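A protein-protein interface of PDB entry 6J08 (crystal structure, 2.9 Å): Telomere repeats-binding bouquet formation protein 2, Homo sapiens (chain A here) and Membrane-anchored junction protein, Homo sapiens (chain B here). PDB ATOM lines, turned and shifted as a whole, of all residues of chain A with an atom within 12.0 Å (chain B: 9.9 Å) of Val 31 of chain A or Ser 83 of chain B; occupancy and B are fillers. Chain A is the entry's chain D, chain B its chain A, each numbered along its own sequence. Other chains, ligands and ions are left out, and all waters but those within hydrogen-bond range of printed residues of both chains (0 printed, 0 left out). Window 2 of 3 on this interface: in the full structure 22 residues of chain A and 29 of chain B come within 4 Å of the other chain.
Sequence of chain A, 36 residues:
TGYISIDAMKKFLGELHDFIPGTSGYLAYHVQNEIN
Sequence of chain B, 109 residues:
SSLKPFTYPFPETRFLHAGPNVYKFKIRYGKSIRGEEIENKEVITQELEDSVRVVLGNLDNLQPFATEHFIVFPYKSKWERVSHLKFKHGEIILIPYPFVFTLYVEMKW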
ATOM      1  N   LEU A  27     -17.139  15.697  -5.143  1.00  0.00           N
ATOM      2  CA  LEU A  27     -18.115  14.914  -4.349  1.00  0.00           C
ATOM      3  C   LEU A  27     -19.089  15.885  -3.699  1.00  0.00           C
ATOM      4  O   LEU A  27     -18.645  16.968  -3.282  1.00  0.00           O
ATOM      5  CB  LEU A  27     -17.378  14.110  -3.279  1.00  0.00           C
ATOM      6  CG  LEU A  27     -16.391  13.059  -3.794  1.00  0.00           C
ATOM      7  CD1 LEU A  27     -15.622  12.466  -2.628  1.00  0.00           C
ATOM      8  CD2 LEU A  27     -17.088  11.963  -4.596  1.00  0.00           C
ATOM      9  N   ALA A  28     -20.362  15.499  -3.672  1.00  0.00           N
ATOM     10  CA  ALA A  28     -21.480  16.204  -3.018  1.00  0.00           C
ATOM     11  C   ALA A  28     -22.036  15.270  -1.951  1.00  0.00           C
ATOM     12  O   ALA A  28     -21.995  14.049  -2.173  1.00  0.00           O
ATOM     13  CB  ALA A  28     -22.535  16.561  -4.035  1.00  0.00           C
ATOM     14  N   TYR A  29     -22.537  15.834  -0.854  1.00  0.00           N
ATOM     15  CA  TYR A  29     -23.019  15.095   0.344  1.00  0.00           C
ATOM     16  C   TYR A  29     -24.359  15.682   0.805  1.00  0.00           C
ATOM     17  O   TYR A  29     -24.486  16.903   0.895  1.00  0.00           O
ATOM     18  CB  TYR A  29     -21.972  15.144   1.465  1.00  0.00           C
ATOM     19  CG  TYR A  29     -20.653  14.482   1.144  1.00  0.00           C
ATOM     20  CD1 TYR A  29     -19.710  15.105   0.344  1.00  0.00           C
ATOM     21  CD2 TYR A  29     -20.354  13.218   1.619  1.00  0.00           C
ATOM     22  CE1 TYR A  29     -18.507  14.495   0.030  1.00  0.00           C
ATOM     23  CE2 TYR A  29     -19.149  12.601   1.331  1.00  0.00           C
ATOM     24  CZ  TYR A  29     -18.220  13.236   0.528  1.00  0.00           C
ATOM     25  OH  TYR A  29     -17.035  12.625   0.229  1.00  0.00           O
ATOM     26  N   HIS A  30     -25.333  14.822   1.093  1.00  0.00           N
ATOM     27  CA  HIS A  30     -26.671  15.219   1.589  1.00  0.00           C
ATOM     28  C   HIS A  30     -26.792  14.798   3.050  1.00  0.00           C
ATOM     29  O   HIS A  30     -26.686  13.593   3.317  1.00  0.00           O
ATOM     30  CB  HIS A  30     -27.790  14.608   0.734  1.00  0.00           C
ATOM     31  CG  HIS A  30     -29.122  15.215   1.024  1.00  0.00           C
ATOM     32  ND1 HIS A  30     -29.843  14.904   2.162  1.00  0.00           N
ATOM     33  CD2 HIS A  30     -29.843  16.149   0.363  1.00  0.00           C
ATOM     34  CE1 HIS A  30     -30.957  15.611   2.181  1.00  0.00           C
ATOM     35  NE2 HIS A  30     -30.982  16.384   1.086  1.00  0.00           N
ATOM     36  N   VAL A  31     -27.033  15.754   3.948  1.00  0.00           N
ATOM     37  CA  VAL A  31     -27.361  15.479   5.377  1.00  0.00           C
ATOM     38  C   VAL A  31     -28.422  14.360   5.432  1.00  0.00           C
ATOM     39  O   VAL A  31     -29.323  14.339   4.567  1.00  0.00           O
ATOM     40  CB  VAL A  31     -27.776  16.774   6.106  1.00  0.00           C
ATOM     41  CG1 VAL A  31     -28.392  16.508   7.471  1.00  0.00           C
ATOM     42  CG2 VAL A  31     -26.591  17.722   6.246  1.00  0.00           C
ATOM     43  N   GLN A  32     -28.245  13.417   6.367  1.00  0.00           N
ATOM     44  CA  GLN A  32     -29.193  12.318   6.708  1.00  0.00           C
ATOM     45  C   GLN A  32     -29.419  12.296   8.225  1.00  0.00           C
ATOM     46  O   GLN A  32     -28.527  12.758   8.975  1.00  0.00           O
ATOM     47  CB  GLN A  32     -28.647  10.951   6.291  1.00  0.00           C
ATOM     48  CG  GLN A  32     -28.561  10.747   4.788  1.00  0.00           C
ATOM     49  CD  GLN A  32     -28.092   9.353   4.452  1.00  0.00           C
ATOM     50  OE1 GLN A  32     -27.412   8.691   5.240  1.00  0.00           O
ATOM     51  NE2 GLN A  32     -28.450   8.896   3.263  1.00  0.00           N
ATOM     52  N   ASN A  33     -30.570  11.765   8.647  1.00  0.00           N
ATOM     53  CA  ASN A  33     -30.945  11.557  10.072  1.00  0.00           C
ATOM     54  C   ASN A  33     -31.225  10.062  10.308  1.00  0.00           C
ATOM     55  O   ASN A  33     -31.723   9.712  11.395  1.00  0.00           O
ATOM     56  CB  ASN A  33     -32.095  12.493  10.453  1.00  0.00           C
ATOM     57  CG  ASN A  33     -31.719  13.954  10.302  1.00  0.00           C
ATOM     58  OD1 ASN A  33     -31.163  14.553  11.223  1.00  0.00           O
ATOM     59  ND2 ASN A  33     -32.007  14.533   9.144  1.00  0.00           N
ATOM     60  N   GLU A  34     -30.897   9.219   9.324  1.00  0.00           N
ATOM     61  CA  GLU A  34     -30.856   7.738   9.427  1.00  0.00           C
ATOM     62  C   GLU A  34     -29.556   7.248   8.787  1.00  0.00           C
ATOM     63  O   GLU A  34     -29.097   7.892   7.819  1.00  0.00           O
ATOM     64  CB  GLU A  34     -32.031   7.094   8.699  1.00  0.00           C
ATOM     65  CG  GLU A  34     -33.384   7.553   9.194  1.00  0.00           C
ATOM     66  CD  GLU A  34     -34.531   6.809   8.536  1.00  0.00           C
ATOM     67  OE1 GLU A  34     -34.257   5.859   7.774  1.00  0.00           O
ATOM     68  OE2 GLU A  34     -35.694   7.177   8.781  1.00  0.00           O
ATOM     69  N   ILE A  35     -28.993   6.154   9.301  1.00  0.00           N
ATOM     70  CA  ILE A  35     -27.703   5.591   8.806  1.00  0.00           C
ATOM     71  C   ILE A  35     -27.913   4.106   8.477  1.00  0.00           C
ATOM     72  O   ILE A  35     -28.778   3.467   9.115  1.00  0.00           O
ATOM     73  CB  ILE A  35     -26.570   5.834   9.827  1.00  0.00           C
ATOM     74  CG1 ILE A  35     -26.660   7.221  10.477  1.00  0.00           C
ATOM     75  CG2 ILE A  35     -25.215   5.602   9.168  1.00  0.00           C
ATOM     76  CD1 ILE A  35     -25.684   7.449  11.610  1.00  0.00           C
ATOM     77  N   ASN A  36     -27.175   3.602   7.482  1.00  0.00           N
ATOM     78  CA  ASN A  36     -27.105   2.159   7.128  1.00  0.00           C
ATOM     79  C   ASN A  36     -25.752   1.871   6.457  1.00  0.00           C
ATOM     80  O   ASN A  36     -24.595   2.318   7.030  1.00  0.00           O
ATOM     81  CB  ASN A  36     -28.300   1.739   6.264  1.00  0.00           C
ATOM     82  CG  ASN A  36     -28.426   0.236   6.110  1.00  0.00           C
ATOM     83  OD1 ASN A  36     -27.439  -0.462   5.883  1.00  0.00           O
ATOM     84  ND2 ASN A  36     -29.640  -0.278   6.229  1.00  0.00           N
ATOM     85  N   LYS B  78     -33.654  32.294  -3.824  1.00  0.00           N
ATOM     86  CA  LYS B  78     -33.039  31.574  -2.679  1.00  0.00           C
ATOM     87  C   LYS B  78     -32.882  30.107  -3.062  1.00  0.00           C
ATOM     88  O   LYS B  78     -33.772  29.557  -3.764  1.00  0.00           O
ATOM     89  CB  LYS B  78     -33.897  31.656  -1.417  1.00  0.00           C
ATOM     90  CG  LYS B  78     -33.311  30.987  -0.183  1.00  0.00           C
ATOM     91  CD  LYS B  78     -34.051  31.364   1.089  1.00  0.00           C
ATOM     92  CE  LYS B  78     -33.506  30.682   2.323  1.00  0.00           C
ATOM     93  NZ  LYS B  78     -34.243  31.118   3.528  1.00  0.00           N
ATOM     94  N   TRP B  79     -31.754  29.533  -2.651  1.00  0.00           N
ATOM     95  CA  TRP B  79     -31.445  28.089  -2.774  1.00  0.00           C
ATOM     96  C   TRP B  79     -31.943  27.393  -1.502  1.00  0.00           C
ATOM     97  O   TRP B  79     -31.393  27.633  -0.401  1.00  0.00           O
ATOM     98  CB  TRP B  79     -29.949  27.930  -3.010  1.00  0.00           C
ATOM     99  CG  TRP B  79     -29.516  26.545  -3.371  1.00  0.00           C
ATOM    100  CD1 TRP B  79     -30.182  25.364  -3.197  1.00  0.00           C
ATOM    101  CD2 TRP B  79     -28.231  26.200  -3.908  1.00  0.00           C
ATOM    102  NE1 TRP B  79     -29.407  24.314  -3.612  1.00  0.00           N
ATOM    103  CE2 TRP B  79     -28.207  24.801  -4.059  1.00  0.00           C
ATOM    104  CE3 TRP B  79     -27.108  26.948  -4.264  1.00  0.00           C
ATOM    105  CZ2 TRP B  79     -27.100  24.139  -4.576  1.00  0.00           C
ATOM    106  CZ3 TRP B  79     -26.006  26.291  -4.760  1.00  0.00           C
ATOM    107  CH2 TRP B  79     -26.005  24.905  -4.904  1.00  0.00           C
ATOM    108  N   GLU B  80     -33.027  26.636  -1.634  1.00  0.00           N
ATOM    109  CA  GLU B  80     -33.745  26.066  -0.473  1.00  0.00           C
ATOM    110  C   GLU B  80     -32.975  24.817  -0.025  1.00  0.00           C
ATOM    111  O   GLU B  80     -32.603  24.015  -0.904  1.00  0.00           O
ATOM    112  CB  GLU B  80     -35.219  25.844  -0.840  1.00  0.00           C
ATOM    113  CG  GLU B  80     -36.047  27.127  -0.857  1.00  0.00           C
ATOM    114  CD  GLU B  80     -36.098  27.935   0.441  1.00  0.00           C
ATOM    115  OE1 GLU B  80     -35.741  27.394   1.516  1.00  0.00           O
ATOM    116  OE2 GLU B  80     -36.499  29.120   0.380  1.00  0.00           O
ATOM    117  N   ARG B  81     -32.687  24.705   1.278  1.00  0.00           N
ATOM    118  CA  ARG B  81     -32.003  23.530   1.892  1.00  0.00           C
ATOM    119  C   ARG B  81     -30.558  23.407   1.377  1.00  0.00           C
ATOM    120  O   ARG B  81     -30.190  22.309   0.937  1.00  0.00           O
ATOM    121  CB  ARG B  81     -32.778  22.248   1.565  1.00  0.00           C
ATOM    122  CG  ARG B  81     -34.261  22.288   1.913  1.00  0.00           C
ATOM    123  CD  ARG B  81     -34.997  21.102   1.315  1.00  0.00           C
ATOM    124  NE  ARG B  81     -36.310  20.885   1.912  1.00  0.00           N
ATOM    125  CZ  ARG B  81     -37.159  19.922   1.550  1.00  0.00           C
ATOM    126  NH1 ARG B  81     -36.844  19.080   0.578  1.00  0.00           N
ATOM    127  NH2 ARG B  81     -38.330  19.805   2.155  1.00  0.00           N
ATOM    128  N   VAL B  82     -29.781  24.493   1.416  1.00  0.00           N
ATOM    129  CA  VAL B  82     -28.332  24.511   1.056  1.00  0.00           C
ATOM    130  C   VAL B  82     -27.530  23.951   2.227  1.00  0.00           C
ATOM    131  O   VAL B  82     -26.492  23.335   1.970  1.00  0.00           O
ATOM    132  CB  VAL B  82     -27.817  25.919   0.708  1.00  0.00           C
ATOM    133  CG1 VAL B  82     -26.297  26.008   0.753  1.00  0.00           C
ATOM    134  CG2 VAL B  82     -28.306  26.358  -0.641  1.00  0.00           C
ATOM    135  N   SER B  83     -27.962  24.226   3.460  1.00  0.00           N
ATOM    136  CA  SER B  83     -27.336  23.703   4.701  1.00  0.00           C
ATOM    137  C   SER B  83     -27.324  22.170   4.652  1.00  0.00           C
ATOM    138  O   SER B  83     -26.439  21.588   5.278  1.00  0.00           O
ATOM    139  CB  SER B  83     -28.023  24.235   5.931  1.00  0.00           C
ATOM    140  OG  SER B  83     -29.394  23.874   5.930  1.00  0.00           O
ATOM    141  N   HIS B  84     -28.240  21.554   3.896  1.00  0.00           N
ATOM    142  CA  HIS B  84     -28.349  20.084   3.695  1.00  0.00           C
ATOM    143  C   HIS B  84     -27.193  19.547   2.843  1.00  0.00           C
ATOM    144  O   HIS B  84     -27.033  18.318   2.795  1.00  0.00           O
ATOM    145  CB  HIS B  84     -29.672  19.708   3.016  1.00  0.00           C
ATOM    146  CG  HIS B  84     -30.880  19.902   3.865  1.00  0.00           C
ATOM    147  ND1 HIS B  84     -32.102  19.312   3.555  1.00  0.00           N
ATOM    148  CD2 HIS B  84     -31.062  20.601   5.008  1.00  0.00           C
ATOM    149  CE1 HIS B  84     -32.990  19.663   4.463  1.00  0.00           C
ATOM    150  NE2 HIS B  84     -32.378  20.453   5.364  1.00  0.00           N
ATOM    151  N   LEU B  85     -26.436  20.410   2.173  1.00  0.00           N
ATOM    152  CA  LEU B  85     -25.452  19.984   1.147  1.00  0.00           C
ATOM    153  C   LEU B  85     -24.041  20.449   1.512  1.00  0.00           C
ATOM    154  O   LEU B  85     -23.868  21.601   1.975  1.00  0.00           O
ATOM    155  CB  LEU B  85     -25.851  20.560  -0.215  1.00  0.00           C
ATOM    156  CG  LEU B  85     -27.168  20.066  -0.808  1.00  0.00           C
ATOM    157  CD1 LEU B  85     -27.441  20.790  -2.113  1.00  0.00           C
ATOM    158  CD2 LEU B  85     -27.163  18.558  -1.030  1.00  0.00           C
ATOM    159  N   LYS B  86     -23.068  19.577   1.247  1.00  0.00           N
ATOM    160  CA  LYS B  86     -21.618  19.889   1.279  1.00  0.00           C
ATOM    161  C   LYS B  86     -21.035  19.483  -0.073  1.00  0.00           C
ATOM    162  O   LYS B  86     -21.395  18.417  -0.600  1.00  0.00           O
ATOM    163  CB  LYS B  86     -20.903  19.189   2.438  1.00  0.00           C
ATOM    164  CG  LYS B  86     -21.521  19.404   3.818  1.00  0.00           C
ATOM    165  CD  LYS B  86     -21.269  20.780   4.418  1.00  0.00           C
ATOM    166  CE  LYS B  86     -21.882  20.969   5.795  1.00  0.00           C
ATOM    167  NZ  LYS B  86     -21.874  22.397   6.201  1.00  0.00           N
ATOM    168  N   PHE B  87     -20.200  20.349  -0.630  1.00  0.00           N
ATOM    169  CA  PHE B  87     -19.504  20.129  -1.912  1.00  0.00           C
ATOM    170  C   PHE B  87     -18.021  20.070  -1.578  1.00  0.00           C
ATOM    171  O   PHE B  87     -17.582  20.888  -0.748  1.00  0.00           O
ATOM    172  CB  PHE B  87     -19.855  21.248  -2.898  1.00  0.00           C
ATOM    173  CG  PHE B  87     -21.324  21.383  -3.219  1.00  0.00           C
ATOM    174  CD1 PHE B  87     -22.208  21.980  -2.325  1.00  0.00           C
ATOM    175  CD2 PHE B  87     -21.825  20.938  -4.432  1.00  0.00           C
ATOM    176  CE1 PHE B  87     -23.554  22.115  -2.635  1.00  0.00           C
ATOM    177  CE2 PHE B  87     -23.170  21.079  -4.745  1.00  0.00           C
ATOM    178  CZ  PHE B  87     -24.033  21.665  -3.844  1.00  0.00           C
ATOM    179  N   PRO B  96     -21.104  27.041  -1.139  1.00  0.00           N
ATOM    180  CA  PRO B  96     -22.267  27.224  -1.999  1.00  0.00           C
ATOM    181  C   PRO B  96     -22.689  28.693  -2.015  1.00  0.00           C
ATOM    182  O   PRO B  96     -22.826  29.295  -0.941  1.00  0.00           O
ATOM    183  CB  PRO B  96     -23.360  26.362  -1.350  1.00  0.00           C
ATOM    184  CG  PRO B  96     -22.594  25.426  -0.464  1.00  0.00           C
ATOM    185  CD  PRO B  96     -21.436  26.256   0.049  1.00  0.00           C
ATOM    186  N   TYR B  97     -22.865  29.258  -3.202  1.00  0.00           N
ATOM    187  CA  TYR B  97     -23.513  30.585  -3.286  1.00  0.00           C
ATOM    188  C   TYR B  97     -25.005  30.314  -3.159  1.00  0.00           C
ATOM    189  O   TYR B  97     -25.571  29.682  -4.044  1.00  0.00           O
ATOM    190  CB  TYR B  97     -23.094  31.359  -4.528  1.00  0.00           C
ATOM    191  CG  TYR B  97     -23.649  32.753  -4.510  1.00  0.00           C
ATOM    192  CD1 TYR B  97     -23.212  33.682  -3.582  1.00  0.00           C
ATOM    193  CD2 TYR B  97     -24.656  33.136  -5.382  1.00  0.00           C
ATOM    194  CE1 TYR B  97     -23.751  34.956  -3.530  1.00  0.00           C
ATOM    195  CE2 TYR B  97     -25.181  34.420  -5.366  1.00  0.00           C
ATOM    196  CZ  TYR B  97     -24.730  35.329  -4.431  1.00  0.00           C
ATOM    197  OH  TYR B  97     -25.268  36.577  -4.398  1.00  0.00           O
ATOM    198  N   PRO B  98     -25.647  30.714  -2.029  1.00  0.00           N
ATOM    199  CA  PRO B  98     -26.959  30.195  -1.634  1.00  0.00           C
ATOM    200  C   PRO B  98     -28.124  30.844  -2.390  1.00  0.00           C
ATOM    201  O   PRO B  98     -29.059  31.295  -1.741  1.00  0.00           O
ATOM    202  CB  PRO B  98     -27.007  30.568  -0.154  1.00  0.00           C
ATOM    203  CG  PRO B  98     -26.326  31.897  -0.132  1.00  0.00           C
ATOM    204  CD  PRO B  98     -25.149  31.704  -1.059  1.00  0.00           C
ATOM    205  N   PHE B  99     -27.999  30.879  -3.721  1.00  0.00           N
ATOM    206  CA  PHE B  99     -28.988  31.383  -4.707  1.00  0.00           C
ATOM    207  C   PHE B  99     -28.914  30.553  -5.976  1.00  0.00           C
ATOM    208  O   PHE B  99     -27.808  30.193  -6.432  1.00  0.00           O
ATOM    209  CB  PHE B  99     -28.724  32.839  -5.081  1.00  0.00           C
ATOM    210  CG  PHE B  99     -28.991  33.773  -3.933  1.00  0.00           C
ATOM    211  CD1 PHE B  99     -27.989  34.056  -3.014  1.00  0.00           C
ATOM    212  CD2 PHE B  99     -30.263  34.273  -3.703  1.00  0.00           C
ATOM    213  CE1 PHE B  99     -28.241  34.877  -1.927  1.00  0.00           C
ATOM    214  CE2 PHE B  99     -30.507  35.090  -2.616  1.00  0.00           C
ATOM    215  CZ  PHE B  99     -29.498  35.387  -1.729  1.00  0.00           C
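The backbone carbonyl oxygen (O) of His 84 of chain B lies within hydrogen-bond range of the backbone NH (N) of Val 31 of chain A. The backbone NH (N) of Tyr 29 of chain A is in hydrogen-bond range of the backbone carbonyl oxygen (O) of Lys 86 of chain B, at 2.8 Å. The backbone carbonyl oxygen of Tyr 29 of chain A sits close to the backbone carbonyl oxygen of His 84 of chain B, 3.5 Å away.
Among the printed residues, merely in contact across the chains: Leu 27 of chain A with Phe 87 of chain B, Ala 28 of chain A with Lys 86 of chain B, Tyr 29 of chain A with Leu 85 of chain B, His 30 of chain A with His 84 of chain B, His 30 of chain A with Leu 85 of chain B and Val 31 of chain A with Ser 83 of chain B.
Of the printed residues of chain B, Leu 27 of chain A touches Phe 87 (3.6 Å). Of the printed residues of chain B, Ala 28 of chain A touches Lys 86. Printed residues of chain B within 4 Å of Tyr 29 of chain A: His 84, Leu 85 and Lys 86. His 30 of chain A touches just these residues of chain B: His 84 and Leu 85. Gln 32 of chain A touches none of the printed residues of chain B. Printed residues of chain A within 4 Å of Ser 83 of chain B: Val 31 (3.99 Å). Leu 85 of chain B touches two residues of chain A. Of chain A, only Ala 28 and Tyr 29 come within 4 Å of Lys 86 of chain B. Printed residues of chain A within 4 Å of Phe 87 of chain B: Leu 27 (3.6 Å). The nearest printed residue of chain B that does not touch Val 31 of chain A is Leu 85 of chain B (4.9 Å). The nearest printed residue of chain A that does not touch Ser 83 of chain B is Tyr 29 of chain A (6.7 Å).
Hydrophobic or aromatic side chains of chain A that line the printed part of chain B: Tyr 29, His 30 and Val 31. Printed residues of chain B that touch a printed residue of chain A: Ser 83, His 84, Leu 85, Lys 86 and Phe 87. Hydrophobic or aromatic side chains of chain B within 4 Å of the printed part of chain A: His 84 and Leu 85. Among the printed residues, no Asp or Glu carboxylate lies within 4 Å of a Lys or Arg side-chain nitrogen of the other chain.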
